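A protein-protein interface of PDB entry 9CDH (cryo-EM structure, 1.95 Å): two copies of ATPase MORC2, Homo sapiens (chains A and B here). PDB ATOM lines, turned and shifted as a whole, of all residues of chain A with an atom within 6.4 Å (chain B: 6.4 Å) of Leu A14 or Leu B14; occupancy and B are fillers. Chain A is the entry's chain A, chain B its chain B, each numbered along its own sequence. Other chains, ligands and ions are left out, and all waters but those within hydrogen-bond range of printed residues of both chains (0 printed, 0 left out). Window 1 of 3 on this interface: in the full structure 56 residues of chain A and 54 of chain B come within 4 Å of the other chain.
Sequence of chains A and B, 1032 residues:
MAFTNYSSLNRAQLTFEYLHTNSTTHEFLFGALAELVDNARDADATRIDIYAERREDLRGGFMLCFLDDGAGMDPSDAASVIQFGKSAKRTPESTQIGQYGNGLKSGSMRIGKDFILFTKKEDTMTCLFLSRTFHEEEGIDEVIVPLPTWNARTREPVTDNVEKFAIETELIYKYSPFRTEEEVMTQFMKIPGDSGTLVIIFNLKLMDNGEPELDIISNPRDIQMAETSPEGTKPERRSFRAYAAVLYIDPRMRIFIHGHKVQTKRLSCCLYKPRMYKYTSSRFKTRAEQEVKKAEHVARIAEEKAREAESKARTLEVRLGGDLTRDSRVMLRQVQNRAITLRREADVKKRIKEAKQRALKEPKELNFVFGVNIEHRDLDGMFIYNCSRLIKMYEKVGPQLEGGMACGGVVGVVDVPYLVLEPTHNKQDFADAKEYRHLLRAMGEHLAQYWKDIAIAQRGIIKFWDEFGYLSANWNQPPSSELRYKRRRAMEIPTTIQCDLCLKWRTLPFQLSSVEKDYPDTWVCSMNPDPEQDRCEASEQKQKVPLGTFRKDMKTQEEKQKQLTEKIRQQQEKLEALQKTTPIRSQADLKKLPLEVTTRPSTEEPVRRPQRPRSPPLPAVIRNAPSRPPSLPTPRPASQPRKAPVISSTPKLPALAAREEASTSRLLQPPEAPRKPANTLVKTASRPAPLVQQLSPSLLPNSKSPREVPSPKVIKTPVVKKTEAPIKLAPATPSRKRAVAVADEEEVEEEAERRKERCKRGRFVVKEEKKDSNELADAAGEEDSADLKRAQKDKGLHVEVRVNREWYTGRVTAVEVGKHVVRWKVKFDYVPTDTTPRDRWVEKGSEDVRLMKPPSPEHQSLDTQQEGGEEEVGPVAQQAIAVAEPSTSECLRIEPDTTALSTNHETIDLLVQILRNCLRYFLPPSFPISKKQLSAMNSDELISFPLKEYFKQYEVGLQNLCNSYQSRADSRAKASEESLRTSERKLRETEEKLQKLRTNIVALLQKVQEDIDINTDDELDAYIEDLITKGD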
ATOM      1  N   ARG A  11     -10.638  -9.124  -4.518  1.00  0.00           N
ATOM      2  CA  ARG A  11     -11.693  -8.956  -3.533  1.00  0.00           C
ATOM      3  C   ARG A  11     -12.970  -8.539  -4.242  1.00  0.00           C
ATOM      4  O   ARG A  11     -12.932  -7.751  -5.190  1.00  0.00           O
ATOM      5  CB  ARG A  11     -11.322  -7.899  -2.490  1.00  0.00           C
ATOM      6  CG  ARG A  11     -10.721  -8.458  -1.221  1.00  0.00           C
ATOM      7  CD  ARG A  11      -9.292  -8.893  -1.438  1.00  0.00           C
ATOM      8  NE  ARG A  11      -8.613  -9.163  -0.178  1.00  0.00           N
ATOM      9  CZ  ARG A  11      -7.427  -9.745  -0.078  1.00  0.00           C
ATOM     10  NH1 ARG A  11      -6.748 -10.116  -1.149  1.00  0.00           N
ATOM     11  NH2 ARG A  11      -6.909  -9.957   1.127  1.00  0.00           N
ATOM     12  N   ALA A  12     -14.098  -9.077  -3.793  1.00  0.00           N
ATOM     13  CA  ALA A  12     -15.374  -8.542  -4.233  1.00  0.00           C
ATOM     14  C   ALA A  12     -15.496  -7.102  -3.752  1.00  0.00           C
ATOM     15  O   ALA A  12     -15.155  -6.783  -2.610  1.00  0.00           O
ATOM     16  CB  ALA A  12     -16.530  -9.385  -3.698  1.00  0.00           C
ATOM     17  N   GLN A  13     -15.976  -6.228  -4.628  1.00  0.00           N
ATOM     18  CA  GLN A  13     -16.022  -4.804  -4.340  1.00  0.00           C
ATOM     19  C   GLN A  13     -17.427  -4.269  -4.556  1.00  0.00           C
ATOM     20  O   GLN A  13     -18.218  -4.834  -5.315  1.00  0.00           O
ATOM     21  CB  GLN A  13     -15.041  -4.016  -5.216  1.00  0.00           C
ATOM     22  CG  GLN A  13     -13.651  -4.611  -5.299  1.00  0.00           C
ATOM     23  CD  GLN A  13     -12.653  -3.863  -4.452  1.00  0.00           C
ATOM     24  OE1 GLN A  13     -12.643  -3.989  -3.229  1.00  0.00           O
ATOM     25  NE2 GLN A  13     -11.804  -3.074  -5.097  1.00  0.00           N
ATOM     26  N   LEU A  14     -17.726  -3.175  -3.866  1.00  0.00           N
ATOM     27  CA  LEU A  14     -18.967  -2.450  -4.085  1.00  0.00           C
ATOM     28  C   LEU A  14     -18.748  -1.377  -5.139  1.00  0.00           C
ATOM     29  O   LEU A  14     -17.766  -0.632  -5.085  1.00  0.00           O
ATOM     30  CB  LEU A  14     -19.453  -1.808  -2.788  1.00  0.00           C
ATOM     31  CG  LEU A  14     -19.917  -2.770  -1.704  1.00  0.00           C
ATOM     32  CD1 LEU A  14     -20.032  -2.060  -0.378  1.00  0.00           C
ATOM     33  CD2 LEU A  14     -21.239  -3.390  -2.087  1.00  0.00           C
ATOM     34  N   THR A  15     -19.657  -1.305  -6.099  1.00  0.00           N
ATOM     35  CA  THR A  15     -19.669  -0.238  -7.081  1.00  0.00           C
ATOM     36  C   THR A  15     -20.772   0.749  -6.730  1.00  0.00           C
ATOM     37  O   THR A  15     -21.677   0.449  -5.948  1.00  0.00           O
ATOM     38  CB  THR A  15     -19.875  -0.785  -8.496  1.00  0.00           C
ATOM     39  OG1 THR A  15     -21.128  -1.476  -8.569  1.00  0.00           O
ATOM     40  CG2 THR A  15     -18.753  -1.740  -8.861  1.00  0.00           C
ATOM     41  N   PHE A  16     -20.685   1.941  -7.321  1.00  0.00           N
ATOM     42  CA  PHE A  16     -21.662   2.978  -7.018  1.00  0.00           C
ATOM     43  C   PHE A  16     -23.076   2.499  -7.312  1.00  0.00           C
ATOM     44  O   PHE A  16     -23.993   2.720  -6.516  1.00  0.00           O
ATOM     45  CB  PHE A  16     -21.349   4.242  -7.819  1.00  0.00           C
ATOM     46  CG  PHE A  16     -22.522   5.160  -7.977  1.00  0.00           C
ATOM     47  CD1 PHE A  16     -22.889   6.013  -6.955  1.00  0.00           C
ATOM     48  CD2 PHE A  16     -23.263   5.163  -9.145  1.00  0.00           C
ATOM     49  CE1 PHE A  16     -23.970   6.855  -7.095  1.00  0.00           C
ATOM     50  CE2 PHE A  16     -24.345   6.003  -9.289  1.00  0.00           C
ATOM     51  CZ  PHE A  16     -24.699   6.850  -8.263  1.00  0.00           C
ATOM     52  N   TYR A  18     -24.225  -0.321  -7.058  1.00  0.00           N
ATOM     53  CA  TYR A  18     -24.714  -1.279  -6.081  1.00  0.00           C
ATOM     54  C   TYR A  18     -25.512  -0.599  -4.983  1.00  0.00           C
ATOM     55  O   TYR A  18     -26.329  -1.251  -4.334  1.00  0.00           O
ATOM     56  CB  TYR A  18     -23.577  -2.082  -5.462  1.00  0.00           C
ATOM     57  CG  TYR A  18     -24.106  -3.332  -4.801  1.00  0.00           C
ATOM     58  CD1 TYR A  18     -24.585  -4.388  -5.561  1.00  0.00           C
ATOM     59  CD2 TYR A  18     -24.174  -3.436  -3.422  1.00  0.00           C
ATOM     60  CE1 TYR A  18     -25.085  -5.524  -4.968  1.00  0.00           C
ATOM     61  CE2 TYR A  18     -24.673  -4.569  -2.818  1.00  0.00           C
ATOM     62  CZ  TYR A  18     -25.129  -5.610  -3.597  1.00  0.00           C
ATOM     63  OH  TYR A  18     -25.628  -6.744  -3.003  1.00  0.00           O
ATOM     64  N   LEU A  19     -25.300   0.694  -4.748  1.00  0.00           N
ATOM     65  CA  LEU A  19     -26.153   1.392  -3.795  1.00  0.00           C
ATOM     66  C   LEU A  19     -27.607   1.327  -4.241  1.00  0.00           C
ATOM     67  O   LEU A  19     -28.496   0.975  -3.456  1.00  0.00           O
ATOM     68  CB  LEU A  19     -25.691   2.840  -3.634  1.00  0.00           C
ATOM     69  CG  LEU A  19     -24.277   3.013  -3.077  1.00  0.00           C
ATOM     70  CD1 LEU A  19     -23.882   4.478  -3.055  1.00  0.00           C
ATOM     71  CD2 LEU A  19     -24.162   2.405  -1.690  1.00  0.00           C
ATOM     72  N   ILE A  82     -20.158   1.273   6.778  1.00  0.00           N
ATOM     73  CA  ILE A  82     -19.983   1.052   5.348  1.00  0.00           C
ATOM     74  C   ILE A  82     -19.275  -0.267   5.059  1.00  0.00           C
ATOM     75  O   ILE A  82     -18.906  -0.531   3.913  1.00  0.00           O
ATOM     76  CB  ILE A  82     -19.246   2.227   4.690  1.00  0.00           C
ATOM     77  CG1 ILE A  82     -17.850   2.401   5.289  1.00  0.00           C
ATOM     78  CG2 ILE A  82     -20.061   3.500   4.847  1.00  0.00           C
ATOM     79  CD1 ILE A  82     -16.990   3.382   4.535  1.00  0.00           C
ATOM     80  N   GLN A  83     -19.070  -1.100   6.076  1.00  0.00           N
ATOM     81  CA  GLN A  83     -18.655  -2.485   5.870  1.00  0.00           C
ATOM     82  C   GLN A  83     -19.923  -3.299   5.667  1.00  0.00           C
ATOM     83  O   GLN A  83     -20.527  -3.798   6.616  1.00  0.00           O
ATOM     84  CB  GLN A  83     -17.842  -2.997   7.052  1.00  0.00           C
ATOM     85  CG  GLN A  83     -16.567  -2.226   7.306  1.00  0.00           C
ATOM     86  CD  GLN A  83     -15.492  -2.537   6.291  1.00  0.00           C
ATOM     87  OE1 GLN A  83     -15.183  -1.720   5.426  1.00  0.00           O
ATOM     88  NE2 GLN A  83     -14.913  -3.726   6.391  1.00  0.00           N
ATOM     89  N   PHE A  84     -20.340  -3.422   4.411  1.00  0.00           N
ATOM     90  CA  PHE A  84     -21.569  -4.139   4.104  1.00  0.00           C
ATOM     91  C   PHE A  84     -21.489  -5.560   4.638  1.00  0.00           C
ATOM     92  O   PHE A  84     -20.486  -6.255   4.445  1.00  0.00           O
ATOM     93  CB  PHE A  84     -21.814  -4.147   2.599  1.00  0.00           C
ATOM     94  CG  PHE A  84     -22.415  -2.879   2.077  1.00  0.00           C
ATOM     95  CD1 PHE A  84     -21.770  -1.667   2.249  1.00  0.00           C
ATOM     96  CD2 PHE A  84     -23.629  -2.896   1.417  1.00  0.00           C
ATOM     97  CE1 PHE A  84     -22.321  -0.502   1.765  1.00  0.00           C
ATOM     98  CE2 PHE A  84     -24.185  -1.733   0.933  1.00  0.00           C
ATOM     99  CZ  PHE A  84     -23.530  -0.536   1.105  1.00  0.00           C
ATOM    100  N   GLY A  85     -22.546  -5.991   5.318  1.00  0.00           N
ATOM    101  CA  GLY A  85     -22.569  -7.279   5.965  1.00  0.00           C
ATOM    102  C   GLY A  85     -22.005  -7.288   7.365  1.00  0.00           C
ATOM    103  O   GLY A  85     -22.232  -8.256   8.100  1.00  0.00           O
ATOM    104  N   ASP A 141     -17.102   5.267  -9.609  1.00  0.00           N
ATOM    105  CA  ASP A 141     -17.816   3.999  -9.604  1.00  0.00           C
ATOM    106  C   ASP A 141     -17.687   3.248  -8.289  1.00  0.00           C
ATOM    107  O   ASP A 141     -18.544   2.414  -7.985  1.00  0.00           O
ATOM    108  CB  ASP A 141     -17.318   3.101 -10.742  1.00  0.00           C
ATOM    109  CG  ASP A 141     -18.275   1.965 -11.047  1.00  0.00           C
ATOM    110  OD1 ASP A 141     -17.861   1.002 -11.727  1.00  0.00           O
ATOM    111  OD2 ASP A 141     -19.442   2.033 -10.607  1.00  0.00           O
ATOM    112  N   GLU A 142     -16.644   3.516  -7.510  1.00  0.00           N
ATOM    113  CA  GLU A 142     -16.569   2.990  -6.160  1.00  0.00           C
ATOM    114  C   GLU A 142     -17.624   3.667  -5.291  1.00  0.00           C
ATOM    115  O   GLU A 142     -18.414   4.494  -5.752  1.00  0.00           O
ATOM    116  CB  GLU A 142     -15.177   3.209  -5.578  1.00  0.00           C
ATOM    117  CG  GLU A 142     -14.091   2.382  -6.221  1.00  0.00           C
ATOM    118  CD  GLU A 142     -12.716   2.745  -5.706  1.00  0.00           C
ATOM    119  OE1 GLU A 142     -12.305   3.909  -5.888  1.00  0.00           O
ATOM    120  OE2 GLU A 142     -12.051   1.872  -5.112  1.00  0.00           O
ATOM    121  N   VAL A 143     -17.642   3.307  -4.019  1.00  0.00           N
ATOM    122  CA  VAL A 143     -18.475   3.979  -3.027  1.00  0.00           C
ATOM    123  C   VAL A 143     -17.515   4.633  -2.040  1.00  0.00           C
ATOM    124  O   VAL A 143     -17.105   4.031  -1.046  1.00  0.00           O
ATOM    125  CB  VAL A 143     -19.441   3.021  -2.329  1.00  0.00           C
ATOM    126  CG1 VAL A 143     -20.358   3.785  -1.393  1.00  0.00           C
ATOM    127  CG2 VAL A 143     -20.249   2.247  -3.357  1.00  0.00           C
ATOM    128  N   ARG B  11     -13.722   3.534   1.610  1.00  0.00           N
ATOM    129  CA  ARG B  11     -14.581   2.902   0.623  1.00  0.00           C
ATOM    130  C   ARG B  11     -15.527   1.943   1.325  1.00  0.00           C
ATOM    131  O   ARG B  11     -15.122   1.215   2.236  1.00  0.00           O
ATOM    132  CB  ARG B  11     -13.764   2.138  -0.421  1.00  0.00           C
ATOM    133  CG  ARG B  11     -13.494   2.914  -1.689  1.00  0.00           C
ATOM    134  CD  ARG B  11     -12.370   3.902  -1.492  1.00  0.00           C
ATOM    135  NE  ARG B  11     -11.936   4.484  -2.755  1.00  0.00           N
ATOM    136  CZ  ARG B  11     -11.159   5.551  -2.857  1.00  0.00           C
ATOM    137  NH1 ARG B  11     -10.693   6.171  -1.787  1.00  0.00           N
ATOM    138  NH2 ARG B  11     -10.838   6.005  -4.064  1.00  0.00           N
ATOM    139  N   ALA B  12     -16.789   1.953   0.915  1.00  0.00           N
ATOM    140  CA  ALA B  12     -17.685   0.888   1.326  1.00  0.00           C
ATOM    141  C   ALA B  12     -17.123  -0.437   0.834  1.00  0.00           C
ATOM    142  O   ALA B  12     -16.623  -0.537  -0.288  1.00  0.00           O
ATOM    143  CB  ALA B  12     -19.090   1.113   0.772  1.00  0.00           C
ATOM    144  N   GLN B  13     -17.196  -1.458   1.679  1.00  0.00           N
ATOM    145  CA  GLN B  13     -16.560  -2.731   1.390  1.00  0.00           C
ATOM    146  C   GLN B  13     -17.518  -3.874   1.678  1.00  0.00           C
ATOM    147  O   GLN B  13     -18.440  -3.748   2.488  1.00  0.00           O
ATOM    148  CB  GLN B  13     -15.280  -2.901   2.207  1.00  0.00           C
ATOM    149  CG  GLN B  13     -14.136  -2.037   1.719  1.00  0.00           C
ATOM    150  CD  GLN B  13     -12.915  -2.138   2.602  1.00  0.00           C
ATOM    151  OE1 GLN B  13     -13.015  -2.085   3.827  1.00  0.00           O
ATOM    152  NE2 GLN B  13     -11.749  -2.287   1.985  1.00  0.00           N
ATOM    153  N   LEU B  14     -17.291  -4.989   0.993  1.00  0.00           N
ATOM    154  CA  LEU B  14     -18.051  -6.208   1.216  1.00  0.00           C
ATOM    155  C   LEU B  14     -17.350  -7.056   2.264  1.00  0.00           C
ATOM    156  O   LEU B  14     -16.135  -7.263   2.194  1.00  0.00           O
ATOM    157  CB  LEU B  14     -18.199  -7.006  -0.078  1.00  0.00           C
ATOM    158  CG  LEU B  14     -19.044  -6.361  -1.168  1.00  0.00           C
ATOM    159  CD1 LEU B  14     -18.807  -7.038  -2.497  1.00  0.00           C
ATOM    160  CD2 LEU B  14     -20.505  -6.423  -0.798  1.00  0.00           C
ATOM    161  N   THR B  15     -18.114  -7.540   3.232  1.00  0.00           N
ATOM    162  CA  THR B  15     -17.627  -8.505   4.200  1.00  0.00           C
ATOM    163  C   THR B  15     -18.163  -9.883   3.843  1.00  0.00           C
ATOM    164  O   THR B  15     -19.112 -10.024   3.070  1.00  0.00           O
ATOM    165  CB  THR B  15     -18.043  -8.127   5.625  1.00  0.00           C
ATOM    166  OG1 THR B  15     -19.467  -8.218   5.753  1.00  0.00           O
ATOM    167  CG2 THR B  15     -17.594  -6.715   5.950  1.00  0.00           C
ATOM    168  N   PHE B  16     -17.535 -10.907   4.421  1.00  0.00           N
ATOM    169  CA  PHE B  16     -17.937 -12.276   4.122  1.00  0.00           C
ATOM    170  C   PHE B  16     -19.415 -12.488   4.415  1.00  0.00           C
ATOM    171  O   PHE B  16     -20.134 -13.097   3.616  1.00  0.00           O
ATOM    172  CB  PHE B  16     -17.085 -13.257   4.927  1.00  0.00           C
ATOM    173  CG  PHE B  16     -17.710 -14.608   5.083  1.00  0.00           C
ATOM    174  CD1 PHE B  16     -17.643 -15.534   4.061  1.00  0.00           C
ATOM    175  CD2 PHE B  16     -18.372 -14.949   6.248  1.00  0.00           C
ATOM    176  CE1 PHE B  16     -18.221 -16.777   4.198  1.00  0.00           C
ATOM    177  CE2 PHE B  16     -18.952 -16.191   6.389  1.00  0.00           C
ATOM    178  CZ  PHE B  16     -18.876 -17.105   5.364  1.00  0.00           C
ATOM    179  N   TYR B  18     -21.731 -10.510   4.166  1.00  0.00           N
ATOM    180  CA  TYR B  18     -22.606  -9.883   3.191  1.00  0.00           C
ATOM    181  C   TYR B  18     -23.004 -10.852   2.092  1.00  0.00           C
ATOM    182  O   TYR B  18     -24.027 -10.647   1.442  1.00  0.00           O
ATOM    183  CB  TYR B  18     -21.969  -8.645   2.573  1.00  0.00           C
ATOM    184  CG  TYR B  18     -23.015  -7.782   1.912  1.00  0.00           C
ATOM    185  CD1 TYR B  18     -23.927  -7.064   2.673  1.00  0.00           C
ATOM    186  CD2 TYR B  18     -23.127  -7.722   0.532  1.00  0.00           C
ATOM    187  CE1 TYR B  18     -24.894  -6.287   2.081  1.00  0.00           C
ATOM    188  CE2 TYR B  18     -24.092  -6.947  -0.070  1.00  0.00           C
ATOM    189  CZ  TYR B  18     -24.976  -6.233   0.709  1.00  0.00           C
ATOM    190  OH  TYR B  18     -25.943  -5.457   0.118  1.00  0.00           O
ATOM    191  N   LEU B  19     -22.222 -11.904   1.857  1.00  0.00           N
ATOM    192  CA  LEU B  19     -22.659 -12.915   0.903  1.00  0.00           C
ATOM    193  C   LEU B  19     -23.983 -13.523   1.346  1.00  0.00           C
ATOM    194  O   LEU B  19     -24.933 -13.615   0.561  1.00  0.00           O
ATOM    195  CB  LEU B  19     -21.586 -13.991   0.744  1.00  0.00           C
ATOM    196  CG  LEU B  19     -20.251 -13.500   0.180  1.00  0.00           C
ATOM    197  CD1 LEU B  19     -19.233 -14.626   0.150  1.00  0.00           C
ATOM    198  CD2 LEU B  19     -20.433 -12.905  -1.205  1.00  0.00           C
ATOM    199  N   ILE B  82     -17.426 -10.090  -9.677  1.00  0.00           N
ATOM    200  CA  ILE B  82     -17.372  -9.812  -8.248  1.00  0.00           C
ATOM    201  C   ILE B  82     -17.351  -8.315  -7.960  1.00  0.00           C
ATOM    202  O   ILE B  82     -17.150  -7.911  -6.811  1.00  0.00           O
ATOM    203  CB  ILE B  82     -16.174 -10.515  -7.590  1.00  0.00           C
ATOM    204  CG1 ILE B  82     -14.856 -10.015  -8.183  1.00  0.00           C
ATOM    205  CG2 ILE B  82     -16.306 -12.020  -7.755  1.00  0.00           C
ATOM    206  CD1 ILE B  82     -13.639 -10.493  -7.434  1.00  0.00           C
ATOM    207  N   GLN B  83     -17.547  -7.483  -8.977  1.00  0.00           N
ATOM    208  CA  GLN B  83     -17.790  -6.057  -8.775  1.00  0.00           C
ATOM    209  C   GLN B  83     -19.288  -5.891  -8.567  1.00  0.00           C
ATOM    210  O   GLN B  83     -20.052  -5.703  -9.512  1.00  0.00           O
ATOM    211  CB  GLN B  83     -17.292  -5.244  -9.962  1.00  0.00           C
ATOM    212  CG  GLN B  83     -15.787  -5.280 -10.140  1.00  0.00           C
ATOM    213  CD  GLN B  83     -15.061  -4.310  -9.233  1.00  0.00           C
ATOM    214  OE1 GLN B  83     -14.100  -4.677  -8.560  1.00  0.00           O
ATOM    215  NE2 GLN B  83     -15.508  -3.060  -9.218  1.00  0.00           N
ATOM    216  N   PHE B  84     -19.712  -5.978  -7.310  1.00  0.00           N
ATOM    217  CA  PHE B  84     -21.132  -5.905  -7.000  1.00  0.00           C
ATOM    218  C   PHE B  84     -21.721  -4.609  -7.535  1.00  0.00           C
ATOM    219  O   PHE B  84     -21.157  -3.528  -7.344  1.00  0.00           O
ATOM    220  CB  PHE B  84     -21.349  -6.005  -5.493  1.00  0.00           C
ATOM    221  CG  PHE B  84     -21.314  -7.407  -4.968  1.00  0.00           C
ATOM    222  CD1 PHE B  84     -20.188  -8.193  -5.125  1.00  0.00           C
ATOM    223  CD2 PHE B  84     -22.410  -7.941  -4.318  1.00  0.00           C
ATOM    224  CE1 PHE B  84     -20.155  -9.480  -4.640  1.00  0.00           C
ATOM    225  CE2 PHE B  84     -22.384  -9.227  -3.832  1.00  0.00           C
ATOM    226  CZ  PHE B  84     -21.255  -9.997  -3.991  1.00  0.00           C
ATOM    227  N   GLY B  85     -22.859  -4.722  -8.211  1.00  0.00           N
ATOM    228  CA  GLY B  85     -23.487  -3.593  -8.848  1.00  0.00           C
ATOM    229  C   GLY B  85     -22.998  -3.312 -10.250  1.00  0.00           C
ATOM    230  O   GLY B  85     -23.658  -2.560 -10.977  1.00  0.00           O
ATOM    231  N   ASP B 141     -12.773 -12.245   6.607  1.00  0.00           N
ATOM    232  CA  ASP B 141     -13.945 -11.384   6.693  1.00  0.00           C
ATOM    233  C   ASP B 141     -14.238 -10.652   5.394  1.00  0.00           C
ATOM    234  O   ASP B 141     -15.397 -10.308   5.144  1.00  0.00           O
ATOM    235  CB  ASP B 141     -13.776 -10.357   7.817  1.00  0.00           C
ATOM    236  CG  ASP B 141     -15.085  -9.696   8.200  1.00  0.00           C
ATOM    237  OD1 ASP B 141     -16.153 -10.239   7.845  1.00  0.00           O
ATOM    238  OD2 ASP B 141     -15.049  -8.632   8.852  1.00  0.00           O
ATOM    239  N   GLU B 142     -13.227 -10.404   4.567  1.00  0.00           N
ATOM    240  CA  GLU B 142     -13.465  -9.898   3.228  1.00  0.00           C
ATOM    241  C   GLU B 142     -14.062 -11.006   2.366  1.00  0.00           C
ATOM    242  O   GLU B 142     -14.357 -12.108   2.835  1.00  0.00           O
ATOM    243  CB  GLU B 142     -12.170  -9.382   2.609  1.00  0.00           C
ATOM    244  CG  GLU B 142     -11.362  -8.471   3.503  1.00  0.00           C
ATOM    245  CD  GLU B 142     -10.125  -7.942   2.813  1.00  0.00           C
ATOM    246  OE1 GLU B 142     -10.244  -6.974   2.033  1.00  0.00           O
ATOM    247  OE2 GLU B 142      -9.033  -8.497   3.047  1.00  0.00           O
ATOM    248  N   VAL B 143     -14.248 -10.707   1.092  1.00  0.00           N
ATOM    249  CA  VAL B 143     -14.670 -11.698   0.109  1.00  0.00           C
ATOM    250  C   VAL B 143     -13.512 -11.843  -0.872  1.00  0.00           C
ATOM    251  O   VAL B 143     -13.420 -11.125  -1.871  1.00  0.00           O
ATOM    252  CB  VAL B 143     -15.967 -11.306  -0.599  1.00  0.00           C
ATOM    253  CG1 VAL B 143     -16.413 -12.412  -1.536  1.00  0.00           C
ATOM    254  CG2 VAL B 143     -17.050 -10.999   0.422  1.00  0.00           C
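The backbone NH of Gln A13 lies within hydrogen-bond range of the backbone carbonyl oxygen of Ile B82 (3.0 Å).
O of Phe B84 lies within hydrogen-bond range of N of Thr A15, 3.0 Å away.
The backbone NH (N) of Phe A84 is in hydrogen-bond range of the backbone carbonyl oxygen (O) of Gln B13.
The backbone NH (N) of Phe B84 sits at hydrogen-bond distance from the backbone carbonyl oxygen (O) of Gln A13.
NH2 of Arg A11 is in salt-bridge range of OE2 of Glu B142, at 3.2 Å.
OH of Tyr A18 lies close to OH of Tyr B18 (3.4 Å).
OE1 of Glu A142 lies within salt-bridge range of NH2 of Arg B11 (3.1 Å).
The backbone carbonyl oxygen of Phe A84 sits at hydrogen-bond distance from the side-chain hydroxyl of Thr B15 (2.6 Å).
N of Gln B13 sits at hydrogen-bond distance from O of Ile A82 (3.0 Å).
The backbone NH of Ala A12 sits at hydrogen-bond distance from the backbone carbonyl oxygen of Val B143 (2.9 Å).
OE1 of Gln B13 sits close to OE1 of Gln A83 (2.7 Å).
The backbone carbonyl oxygen (O) of Val A143 is in hydrogen-bond range of the backbone NH (N) of Ala B12.
Among the printed residues, pairs that only touch across the chains: Arg A11 with Ile B82, Arg A11 with Val B143, Ala A12 with Leu B14, Ala A12 with Ile B82, Ala A12 with Phe B84, Gln A13 with Leu B14, Gln A13 with Gln B83, Leu A14 with Ala B12, Leu A14 with Gln B13, Leu A14 with Leu B14, Leu A14 with Phe B84, Thr A15 with Gln B83, Thr A15 with Gly B85, Tyr A18 with Phe B84, Tyr A18 with Gly B85, Ile A82 with Arg B11, Ile A82 with Ala B12, Gln A83 with Thr B15, Phe A84 with Ala B12, Phe A84 with Leu B14, Phe A84 with Tyr B18, Gly A85 with Thr B15, Gly A85 with Tyr B18 and Val A143 with Arg B11.
Of the printed residues of chain B, Ala A12 touches Leu B14 (3.5 Å), Ile B82 (3.2 Å), Phe B84 (3.7 Å) and Val B143 (2.9 Å).
Of the printed residues of chain B, Leu A14 touches Ala B12, Gln B13, Leu B14 and Phe B84.
Of the printed residues of chain B, Tyr A18 touches Tyr B18 (3.3 Å), Phe B84 (3.4 Å) and Gly B85 (3.2 Å).
Printed residues of chain B within 4 Å of Ile A82: Arg B11, Ala B12 and Gln B13.
Asp A141 touches none of the printed residues of chain B.
Leu B14 touches just these residues of chain A: Ala A12, Gln A13, Leu A14 and Phe A84.
Leu B19 touches none of the printed residues of chain A.
Of the printed residues of chain A, Glu B142 touches Arg A11.
Printed residues of chain A within 4 Å of Val B143: Arg A11 (3.2 Å) and Ala A12 (2.9 Å).
The nearest residue of chain B that does not touch Leu A14 is Tyr B18 (5.0 Å).
The nearest printed residue of chain B that does not touch Gln A83 is Arg B11 (4.3 Å).
Of the 15 printed residues of chain A, 12 touch a printed residue of chain B.
Printed residues of chain B that touch a printed residue of chain A: Arg B11, Ala B12, Gln B13, Leu B14, Thr B15, Tyr B18, Ile B82, Gln B83, Phe B84, Gly B85, Glu B142 and Val B143.
Hydrophobic or aromatic side chains of chain B that line the printed part of chain A: Ala B12, Leu B14, Tyr B18, Ile B82, Phe B84 and Val B143.
Among the printed residues, 36 pairs touch across the chains.
Arg A11 touches Glu B142, and with the chains exchanged Glu A142 touches Arg B11.
Gln A13 touches Gln B83, and with the chains exchanged Gln A83 touches Gln B13.
Leu A14 touches its own counterpart, Leu B14.
Tyr B18 touches its own counterpart, Tyr A18.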
